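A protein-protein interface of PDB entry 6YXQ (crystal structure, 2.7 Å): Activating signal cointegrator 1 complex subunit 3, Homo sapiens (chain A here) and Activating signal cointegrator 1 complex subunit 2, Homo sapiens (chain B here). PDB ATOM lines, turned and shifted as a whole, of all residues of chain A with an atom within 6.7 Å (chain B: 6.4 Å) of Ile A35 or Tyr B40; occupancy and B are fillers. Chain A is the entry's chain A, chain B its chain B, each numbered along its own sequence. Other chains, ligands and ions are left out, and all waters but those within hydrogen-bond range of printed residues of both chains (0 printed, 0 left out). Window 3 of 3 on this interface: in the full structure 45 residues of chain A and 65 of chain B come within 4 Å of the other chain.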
ATOM      1  N   GLU A  28      29.078  16.447  -6.959  1.00  0.00           N
ATOM      2  CA  GLU A  28      27.749  16.006  -7.346  1.00  0.00           C
ATOM      3  C   GLU A  28      27.038  17.228  -7.892  1.00  0.00           C
ATOM      4  O   GLU A  28      26.963  18.249  -7.203  1.00  0.00           O
ATOM      5  CB  GLU A  28      27.019  15.432  -6.130  1.00  0.00           C
ATOM      6  CG  GLU A  28      25.773  14.634  -6.427  1.00  0.00           C
ATOM      7  CD  GLU A  28      25.230  13.957  -5.190  1.00  0.00           C
ATOM      8  OE1 GLU A  28      25.930  13.088  -4.635  1.00  0.00           O
ATOM      9  OE2 GLU A  28      24.123  14.318  -4.746  1.00  0.00           O
ATOM     10  N   VAL A  30      24.035  17.424 -11.254  1.00  0.00           N
ATOM     11  CA  VAL A  30      22.619  17.129 -11.507  1.00  0.00           C
ATOM     12  C   VAL A  30      22.246  15.695 -11.135  1.00  0.00           C
ATOM     13  O   VAL A  30      21.062  15.353 -11.168  1.00  0.00           O
ATOM     14  CB  VAL A  30      22.180  17.449 -12.956  1.00  0.00           C
ATOM     15  CG1 VAL A  30      22.610  16.379 -13.938  1.00  0.00           C
ATOM     16  CG2 VAL A  30      20.652  17.716 -12.993  1.00  0.00           C
ATOM     17  N   ALA A  31      23.195  14.844 -10.746  1.00  0.00           N
ATOM     18  CA  ALA A  31      22.775  13.693  -9.957  1.00  0.00           C
ATOM     19  C   ALA A  31      22.097  14.191  -8.684  1.00  0.00           C
ATOM     20  O   ALA A  31      20.964  13.798  -8.357  1.00  0.00           O
ATOM     21  CB  ALA A  31      23.967  12.790  -9.632  1.00  0.00           C
ATOM     22  N   ASP A  32      22.761  15.144  -8.016  1.00  0.00           N
ATOM     23  CA  ASP A  32      22.277  15.758  -6.782  1.00  0.00           C
ATOM     24  C   ASP A  32      20.859  16.308  -6.926  1.00  0.00           C
ATOM     25  O   ASP A  32      19.957  15.935  -6.169  1.00  0.00           O
ATOM     26  CB  ASP A  32      23.257  16.865  -6.365  1.00  0.00           C
ATOM     27  CG  ASP A  32      22.657  17.873  -5.426  1.00  0.00           C
ATOM     28  OD1 ASP A  32      21.956  17.475  -4.483  1.00  0.00           O
ATOM     29  OD2 ASP A  32      22.881  19.079  -5.651  1.00  0.00           O
ATOM     30  N   LEU A  33      20.642  17.210  -7.891  1.00  0.00           N
ATOM     31  CA  LEU A  33      19.349  17.883  -8.009  1.00  0.00           C
ATOM     32  C   LEU A  33      18.320  16.997  -8.662  1.00  0.00           C
ATOM     33  O   LEU A  33      17.109  17.148  -8.426  1.00  0.00           O
ATOM     34  CB  LEU A  33      19.490  19.159  -8.837  1.00  0.00           C
ATOM     35  CG  LEU A  33      19.348  20.333  -7.905  1.00  0.00           C
ATOM     36  CD1 LEU A  33      19.486  21.633  -8.657  1.00  0.00           C
ATOM     37  CD2 LEU A  33      18.024  20.229  -7.204  1.00  0.00           C
ATOM     38  N   LYS A  34      18.774  16.130  -9.561  1.00  0.00           N
ATOM     39  CA  LYS A  34      17.823  15.252 -10.199  1.00  0.00           C
ATOM     40  C   LYS A  34      17.118  14.338  -9.240  1.00  0.00           C
ATOM     41  O   LYS A  34      15.918  14.081  -9.391  1.00  0.00           O
ATOM     42  CB  LYS A  34      18.462  14.379 -11.247  1.00  0.00           C
ATOM     43  CG  LYS A  34      17.373  13.478 -11.714  1.00  0.00           C
ATOM     44  CD  LYS A  34      17.728  12.918 -12.902  1.00  0.00           C
ATOM     45  CE  LYS A  34      16.831  13.326 -14.097  1.00  0.00           C
ATOM     46  NZ  LYS A  34      16.984  12.170 -15.101  1.00  0.00           N
ATOM     47  N   ILE A  35      17.864  13.715  -8.330  1.00  0.00           N
ATOM     48  CA  ILE A  35      17.121  12.849  -7.426  1.00  0.00           C
ATOM     49  C   ILE A  35      16.102  13.673  -6.634  1.00  0.00           C
ATOM     50  O   ILE A  35      15.021  13.174  -6.297  1.00  0.00           O
ATOM     51  CB  ILE A  35      18.062  12.035  -6.521  1.00  0.00           C
ATOM     52  CG1 ILE A  35      17.283  11.431  -5.348  1.00  0.00           C
ATOM     53  CG2 ILE A  35      19.207  12.880  -6.047  1.00  0.00           C
ATOM     54  CD1 ILE A  35      17.993  10.306  -4.627  1.00  0.00           C
ATOM     55  N   LYS A  36      16.391  14.954  -6.376  1.00  0.00           N
ATOM     56  CA  LYS A  36      15.392  15.827  -5.759  1.00  0.00           C
ATOM     57  C   LYS A  36      14.151  15.937  -6.631  1.00  0.00           C
ATOM     58  O   LYS A  36      13.018  15.824  -6.147  1.00  0.00           O
ATOM     59  CB  LYS A  36      15.974  17.217  -5.513  1.00  0.00           C
ATOM     60  CG  LYS A  36      15.723  17.762  -4.123  1.00  0.00           C
ATOM     61  CD  LYS A  36      14.276  18.058  -3.820  1.00  0.00           C
ATOM     62  CE  LYS A  36      14.192  18.529  -2.385  1.00  0.00           C
ATOM     63  NZ  LYS A  36      12.814  18.794  -1.917  1.00  0.00           N
ATOM     64  N   ARG A  37      14.356  16.183  -7.924  1.00  0.00           N
ATOM     65  CA  ARG A  37      13.234  16.234  -8.857  1.00  0.00           C
ATOM     66  C   ARG A  37      12.475  14.910  -8.878  1.00  0.00           C
ATOM     67  O   ARG A  37      11.244  14.886  -8.999  1.00  0.00           O
ATOM     68  CB  ARG A  37      13.734  16.596 -10.255  1.00  0.00           C
ATOM     69  CG  ARG A  37      14.524  17.894 -10.306  1.00  0.00           C
ATOM     70  CD  ARG A  37      14.525  18.486 -11.707  1.00  0.00           C
ATOM     71  NE  ARG A  37      15.234  19.761 -11.771  1.00  0.00           N
ATOM     72  CZ  ARG A  37      16.468  19.902 -12.245  1.00  0.00           C
ATOM     73  NH1 ARG A  37      17.132  18.845 -12.697  1.00  0.00           N
ATOM     74  NH2 ARG A  37      17.040  21.099 -12.267  1.00  0.00           N
ATOM     75  N   SER A  38      13.201  13.800  -8.741  1.00  0.00           N
ATOM     76  CA  SER A  38      12.600  12.473  -8.747  1.00  0.00           C
ATOM     77  C   SER A  38      11.575  12.316  -7.631  1.00  0.00           C
ATOM     78  O   SER A  38      10.542  11.663  -7.812  1.00  0.00           O
ATOM     79  CB  SER A  38      13.698  11.412  -8.626  1.00  0.00           C
ATOM     80  OG  SER A  38      13.249  10.267  -7.923  1.00  0.00           O
ATOM     81  N   LYS A  39      11.836  12.909  -6.470  1.00  0.00           N
ATOM     82  CA  LYS A  39      10.963  12.723  -5.323  1.00  0.00           C
ATOM     83  C   LYS A  39      10.149  13.957  -4.967  1.00  0.00           C
ATOM     84  O   LYS A  39       9.440  13.934  -3.957  1.00  0.00           O
ATOM     85  CB  LYS A  39      11.782  12.275  -4.105  1.00  0.00           C
ATOM     86  CG  LYS A  39      13.055  13.049  -3.898  1.00  0.00           C
ATOM     87  CD  LYS A  39      13.963  12.341  -2.916  1.00  0.00           C
ATOM     88  CE  LYS A  39      13.888  10.826  -2.962  1.00  0.00           C
ATOM     89  NZ  LYS A  39      14.956  10.236  -2.090  1.00  0.00           N
ATOM     90  N   LEU A  40      10.208  15.025  -5.762  1.00  0.00           N
ATOM     91  CA  LEU A  40       9.435  16.213  -5.416  1.00  0.00           C
ATOM     92  C   LEU A  40       7.956  16.084  -5.752  1.00  0.00           C
ATOM     93  O   LEU A  40       7.210  17.047  -5.540  1.00  0.00           O
ATOM     94  CB  LEU A  40      10.017  17.467  -6.098  1.00  0.00           C
ATOM     95  CG  LEU A  40      10.072  17.689  -7.620  1.00  0.00           C
ATOM     96  CD1 LEU A  40       8.720  17.994  -8.248  1.00  0.00           C
ATOM     97  CD2 LEU A  40      11.038  18.817  -7.940  1.00  0.00           C
ATOM     98  N   GLN A  43       6.083  15.915  -2.455  1.00  0.00           N
ATOM     99  CA  GLN A  43       6.672  16.710  -1.384  1.00  0.00           C
ATOM    100  C   GLN A  43       5.804  17.905  -1.012  1.00  0.00           C
ATOM    101  O   GLN A  43       5.836  18.350   0.142  1.00  0.00           O
ATOM    102  CB  GLN A  43       8.075  17.170  -1.777  1.00  0.00           C
ATOM    103  CG  GLN A  43       9.136  16.091  -1.613  1.00  0.00           C
ATOM    104  CD  GLN A  43      10.533  16.656  -1.443  1.00  0.00           C
ATOM    105  OE1 GLN A  43      10.705  17.821  -1.081  1.00  0.00           O
ATOM    106  NE2 GLN A  43      11.542  15.830  -1.704  1.00  0.00           N
ATOM    107  N   ALA B  37      12.015  10.991   7.632  1.00  0.00           N
ATOM    108  CA  ALA B  37      11.340  11.174   6.359  1.00  0.00           C
ATOM    109  C   ALA B  37      12.325  11.007   5.205  1.00  0.00           C
ATOM    110  O   ALA B  37      13.541  11.151   5.361  1.00  0.00           O
ATOM    111  CB  ALA B  37      10.675  12.548   6.289  1.00  0.00           C
ATOM    112  N   ASP B  38      11.783  10.698   4.032  1.00  0.00           N
ATOM    113  CA  ASP B  38      12.604  10.467   2.854  1.00  0.00           C
ATOM    114  C   ASP B  38      12.860  11.736   2.056  1.00  0.00           C
ATOM    115  O   ASP B  38      13.263  11.649   0.892  1.00  0.00           O
ATOM    116  CB  ASP B  38      11.962   9.411   1.950  1.00  0.00           C
ATOM    117  CG  ASP B  38      12.994   8.553   1.237  1.00  0.00           C
ATOM    118  OD1 ASP B  38      13.515   8.984   0.184  1.00  0.00           O
ATOM    119  OD2 ASP B  38      13.289   7.448   1.737  1.00  0.00           O
ATOM    120  N   ARG B  39      12.645  12.907   2.650  1.00  0.00           N
ATOM    121  CA  ARG B  39      12.864  14.153   1.929  1.00  0.00           C
ATOM    122  C   ARG B  39      14.344  14.334   1.622  1.00  0.00           C
ATOM    123  O   ARG B  39      15.177  14.399   2.532  1.00  0.00           O
ATOM    124  CB  ARG B  39      12.352  15.344   2.729  1.00  0.00           C
ATOM    125  CG  ARG B  39      12.440  16.642   1.955  1.00  0.00           C
ATOM    126  CD  ARG B  39      11.561  17.686   2.590  1.00  0.00           C
ATOM    127  NE  ARG B  39      10.665  18.372   1.670  1.00  0.00           N
ATOM    128  CZ  ARG B  39       9.342  18.354   1.783  1.00  0.00           C
ATOM    129  NH1 ARG B  39       8.589  19.013   0.914  1.00  0.00           N
ATOM    130  NH2 ARG B  39       8.774  17.666   2.764  1.00  0.00           N
ATOM    131  N   TYR B  40      14.663  14.424   0.339  1.00  0.00           N
ATOM    132  CA  TYR B  40      16.018  14.718  -0.089  1.00  0.00           C
ATOM    133  C   TYR B  40      16.345  16.186   0.164  1.00  0.00           C
ATOM    134  O   TYR B  40      15.478  17.060   0.094  1.00  0.00           O
ATOM    135  CB  TYR B  40      16.151  14.395  -1.570  1.00  0.00           C
ATOM    136  CG  TYR B  40      17.542  14.292  -2.120  1.00  0.00           C
ATOM    137  CD1 TYR B  40      18.281  13.121  -1.989  1.00  0.00           C
ATOM    138  CD2 TYR B  40      18.098  15.347  -2.827  1.00  0.00           C
ATOM    139  CE1 TYR B  40      19.552  13.023  -2.520  1.00  0.00           C
ATOM    140  CE2 TYR B  40      19.362  15.260  -3.355  1.00  0.00           C
ATOM    141  CZ  TYR B  40      20.089  14.101  -3.199  1.00  0.00           C
ATOM    142  OH  TYR B  40      21.350  14.021  -3.742  1.00  0.00           O
ATOM    143  N   PHE B  41      17.616  16.452   0.457  1.00  0.00           N
ATOM    144  CA  PHE B  41      18.124  17.802   0.659  1.00  0.00           C
ATOM    145  C   PHE B  41      19.252  18.056  -0.328  1.00  0.00           C
ATOM    146  O   PHE B  41      20.213  17.281  -0.384  1.00  0.00           O
ATOM    147  CB  PHE B  41      18.645  17.994   2.086  1.00  0.00           C
ATOM    148  CG  PHE B  41      17.590  18.361   3.082  1.00  0.00           C
ATOM    149  CD1 PHE B  41      16.840  17.379   3.717  1.00  0.00           C
ATOM    150  CD2 PHE B  41      17.369  19.685   3.412  1.00  0.00           C
ATOM    151  CE1 PHE B  41      15.872  17.719   4.649  1.00  0.00           C
ATOM    152  CE2 PHE B  41      16.409  20.031   4.344  1.00  0.00           C
ATOM    153  CZ  PHE B  41      15.656  19.048   4.962  1.00  0.00           C
ATOM    154  N   VAL B  42      19.147  19.139  -1.098  1.00  0.00           N
ATOM    155  CA  VAL B  42      20.221  19.510  -2.008  1.00  0.00           C
ATOM    156  C   VAL B  42      21.133  20.532  -1.343  1.00  0.00           C
ATOM    157  O   VAL B  42      20.767  21.217  -0.384  1.00  0.00           O
ATOM    158  CB  VAL B  42      19.699  20.044  -3.358  1.00  0.00           C
ATOM    159  CG1 VAL B  42      18.777  19.051  -3.979  1.00  0.00           C
ATOM    160  CG2 VAL B  42      19.016  21.398  -3.188  1.00  0.00           C
ATOM    161  N   LEU B  43      22.345  20.636  -1.876  1.00  0.00           N
ATOM    162  CA  LEU B  43      23.338  21.558  -1.360  1.00  0.00           C
ATOM    163  C   LEU B  43      23.030  22.982  -1.808  1.00  0.00           C
ATOM    164  O   LEU B  43      22.288  23.218  -2.766  1.00  0.00           O
ATOM    165  CB  LEU B  43      24.735  21.152  -1.826  1.00  0.00           C
ATOM    166  CG  LEU B  43      25.090  19.699  -1.527  1.00  0.00           C
ATOM    167  CD1 LEU B  43      25.920  19.120  -2.652  1.00  0.00           C
ATOM    168  CD2 LEU B  43      25.815  19.573  -0.194  1.00  0.00           C
ATOM    169  N   PHE B  65      14.361  24.855  -3.572  1.00  0.00           N
ATOM    170  CA  PHE B  65      14.397  23.521  -2.975  1.00  0.00           C
ATOM    171  C   PHE B  65      14.823  23.589  -1.508  1.00  0.00           C
ATOM    172  O   PHE B  65      14.134  23.066  -0.612  1.00  0.00           O
ATOM    173  CB  PHE B  65      15.337  22.623  -3.761  1.00  0.00           C
ATOM    174  CG  PHE B  65      14.771  22.154  -5.064  1.00  0.00           C
ATOM    175  CD1 PHE B  65      13.507  21.600  -5.117  1.00  0.00           C
ATOM    176  CD2 PHE B  65      15.499  22.271  -6.236  1.00  0.00           C
ATOM    177  CE1 PHE B  65      12.981  21.159  -6.312  1.00  0.00           C
ATOM    178  CE2 PHE B  65      14.977  21.831  -7.438  1.00  0.00           C
ATOM    179  CZ  PHE B  65      13.716  21.275  -7.475  1.00  0.00           C
ATOM    180  N   ASP B  69      12.327  22.868   1.827  1.00  0.00           N
ATOM    181  CA  ASP B  69      12.671  21.788   2.743  1.00  0.00           C
ATOM    182  C   ASP B  69      12.863  22.307   4.165  1.00  0.00           C
ATOM    183  O   ASP B  69      12.429  21.670   5.131  1.00  0.00           O
ATOM    184  CB  ASP B  69      13.921  21.066   2.253  1.00  0.00           C
ATOM    185  CG  ASP B  69      13.713  20.383   0.915  1.00  0.00           C
ATOM    186  OD1 ASP B  69      12.572  19.974   0.613  1.00  0.00           O
ATOM    187  OD2 ASP B  69      14.700  20.249   0.167  1.00  0.00           O
ATOM    188  N   GLN B  84      14.914  13.410  11.802  1.00  0.00           N
ATOM    189  CA  GLN B  84      15.410  13.854  10.506  1.00  0.00           C
ATOM    190  C   GLN B  84      16.837  14.380  10.618  1.00  0.00           C
ATOM    191  O   GLN B  84      17.719  13.967   9.855  1.00  0.00           O
ATOM    192  CB  GLN B  84      14.473  14.917   9.928  1.00  0.00           C
ATOM    193  CG  GLN B  84      14.685  15.202   8.449  1.00  0.00           C
ATOM    194  CD  GLN B  84      14.190  14.083   7.554  1.00  0.00           C
ATOM    195  OE1 GLN B  84      13.407  13.235   7.978  1.00  0.00           O
ATOM    196  NE2 GLN B  84      14.646  14.077   6.308  1.00  0.00           N
ATOM    197  N   ASP B  88      19.346  11.927   8.578  1.00  0.00           N
ATOM    198  CA  ASP B  88      19.449  12.351   7.187  1.00  0.00           C
ATOM    199  C   ASP B  88      20.769  13.084   7.003  1.00  0.00           C
ATOM    200  O   ASP B  88      20.923  14.221   7.456  1.00  0.00           O
ATOM    201  CB  ASP B  88      18.277  13.250   6.802  1.00  0.00           C
ATOM    202  CG  ASP B  88      18.240  13.552   5.319  1.00  0.00           C
ATOM    203  OD1 ASP B  88      19.272  13.372   4.641  1.00  0.00           O
ATOM    204  OD2 ASP B  88      17.177  13.970   4.825  1.00  0.00           O
ATOM    205  N   THR B  90      21.944  14.209   4.180  1.00  0.00           N
ATOM    206  CA  THR B  90      21.788  15.314   3.234  1.00  0.00           C
ATOM    207  C   THR B  90      21.463  16.615   3.955  1.00  0.00           C
ATOM    208  O   THR B  90      21.956  17.682   3.572  1.00  0.00           O
ATOM    209  CB  THR B  90      20.700  14.993   2.202  1.00  0.00           C
ATOM    210  OG1 THR B  90      19.412  14.987   2.831  1.00  0.00           O
ATOM    211  CG2 THR B  90      20.957  13.641   1.557  1.00  0.00           C
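OE1 of Gln A43 sits at hydrogen-bond distance from NZ of Lys A36 (2.5 Å).
The side-chain carboxylate (OD1) of Asp B69 lies within salt-bridge range of the guanidinium group (NE) of Arg B39 (2.7 Å).
Ile A35 touches one residue of chain B.
Of the printed residues of chain A, Tyr B40 touches Glu A28, Asp A32, Ile A35, Lys A36, Lys A39 and Gln A43.
Of the printed residues of chain A, Asp B38 touches Lys A39.
Of the printed residues of chain A, Val B42 touches Asp A32, Leu A33 and Lys A36.
Of the printed residues of chain B, Lys A39 touches Asp B38 (3.0 Å) and Tyr B40 (3.3 Å).
Gln B84 touches none of the printed residues of chain A.
Arg A37 touches none of the printed residues of chain B.
The nearest printed residue of chain B that does not touch Ile A35 is Val B42 (6.5 Å).
The nearest printed residue of chain B that does not touch Lys A36 is Arg B39 (4.2 Å).
OE2 of Glu A28 sits at hydrogen-bond distance from OH of Tyr B40, at 3.0 Å.
O of Asp A32 sits close to OH of Tyr B40.
The side-chain carboxylate of Asp B69 is in salt-bridge range of the side-chain amino group of Lys A36.
The side-chain amino group (NZ) of Lys A39 is in salt-bridge range of the side-chain carboxylate (OD1) of Asp B38, 3.0 Å away.
The side-chain amide oxygen (OE1) of Gln A43 is in hydrogen-bond range of the guanidinium group (NE) of Arg B39.
The side-chain carboxylate (OD1) of Asp B69 lies close to the side-chain amide oxygen (OE1) of Gln A43 (3.3 Å).
Among the printed residues, pairs that only touch across the chains: Lys A36 with Tyr B40, Ile A35 with Tyr B40, Lys A39 with Tyr B40, Lys A36 with Val B42, Leu A33 with Phe B65, Leu A40 with Phe B65, Leu A33 with Val B42, Asp A32 with Val B42, Lys A36 with Phe B65 and Gln A43 with Tyr B40.
Of the 12 printed residues of chain B, 6 touch a printed residue of chain A.
Hydrophobic or aromatic side chains of chain B that line the printed part of chain A: Tyr B40, Val B42 and Phe B65.
Of the 13 printed residues of chain A, 8 touch a printed residue of chain B.
Printed residues of chain A that touch a printed residue of chain B: Glu A28, Asp A32, Leu A33, Ile A35, Lys A36, Lys A39, Leu A40 and Gln A43.
Hydrophobic or aromatic side chains of chain A within 4 Å of the printed part of chain B: Leu A33, Ile A35 and Leu A40.
Among the printed residues, Asp or Glu carboxylates within 4 Å of a Lys or Arg side-chain nitrogen of the other chain: Lys A36 with Asp B69 (2.8 Å) and Lys A39 with Asp B38 (3.0 Å).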
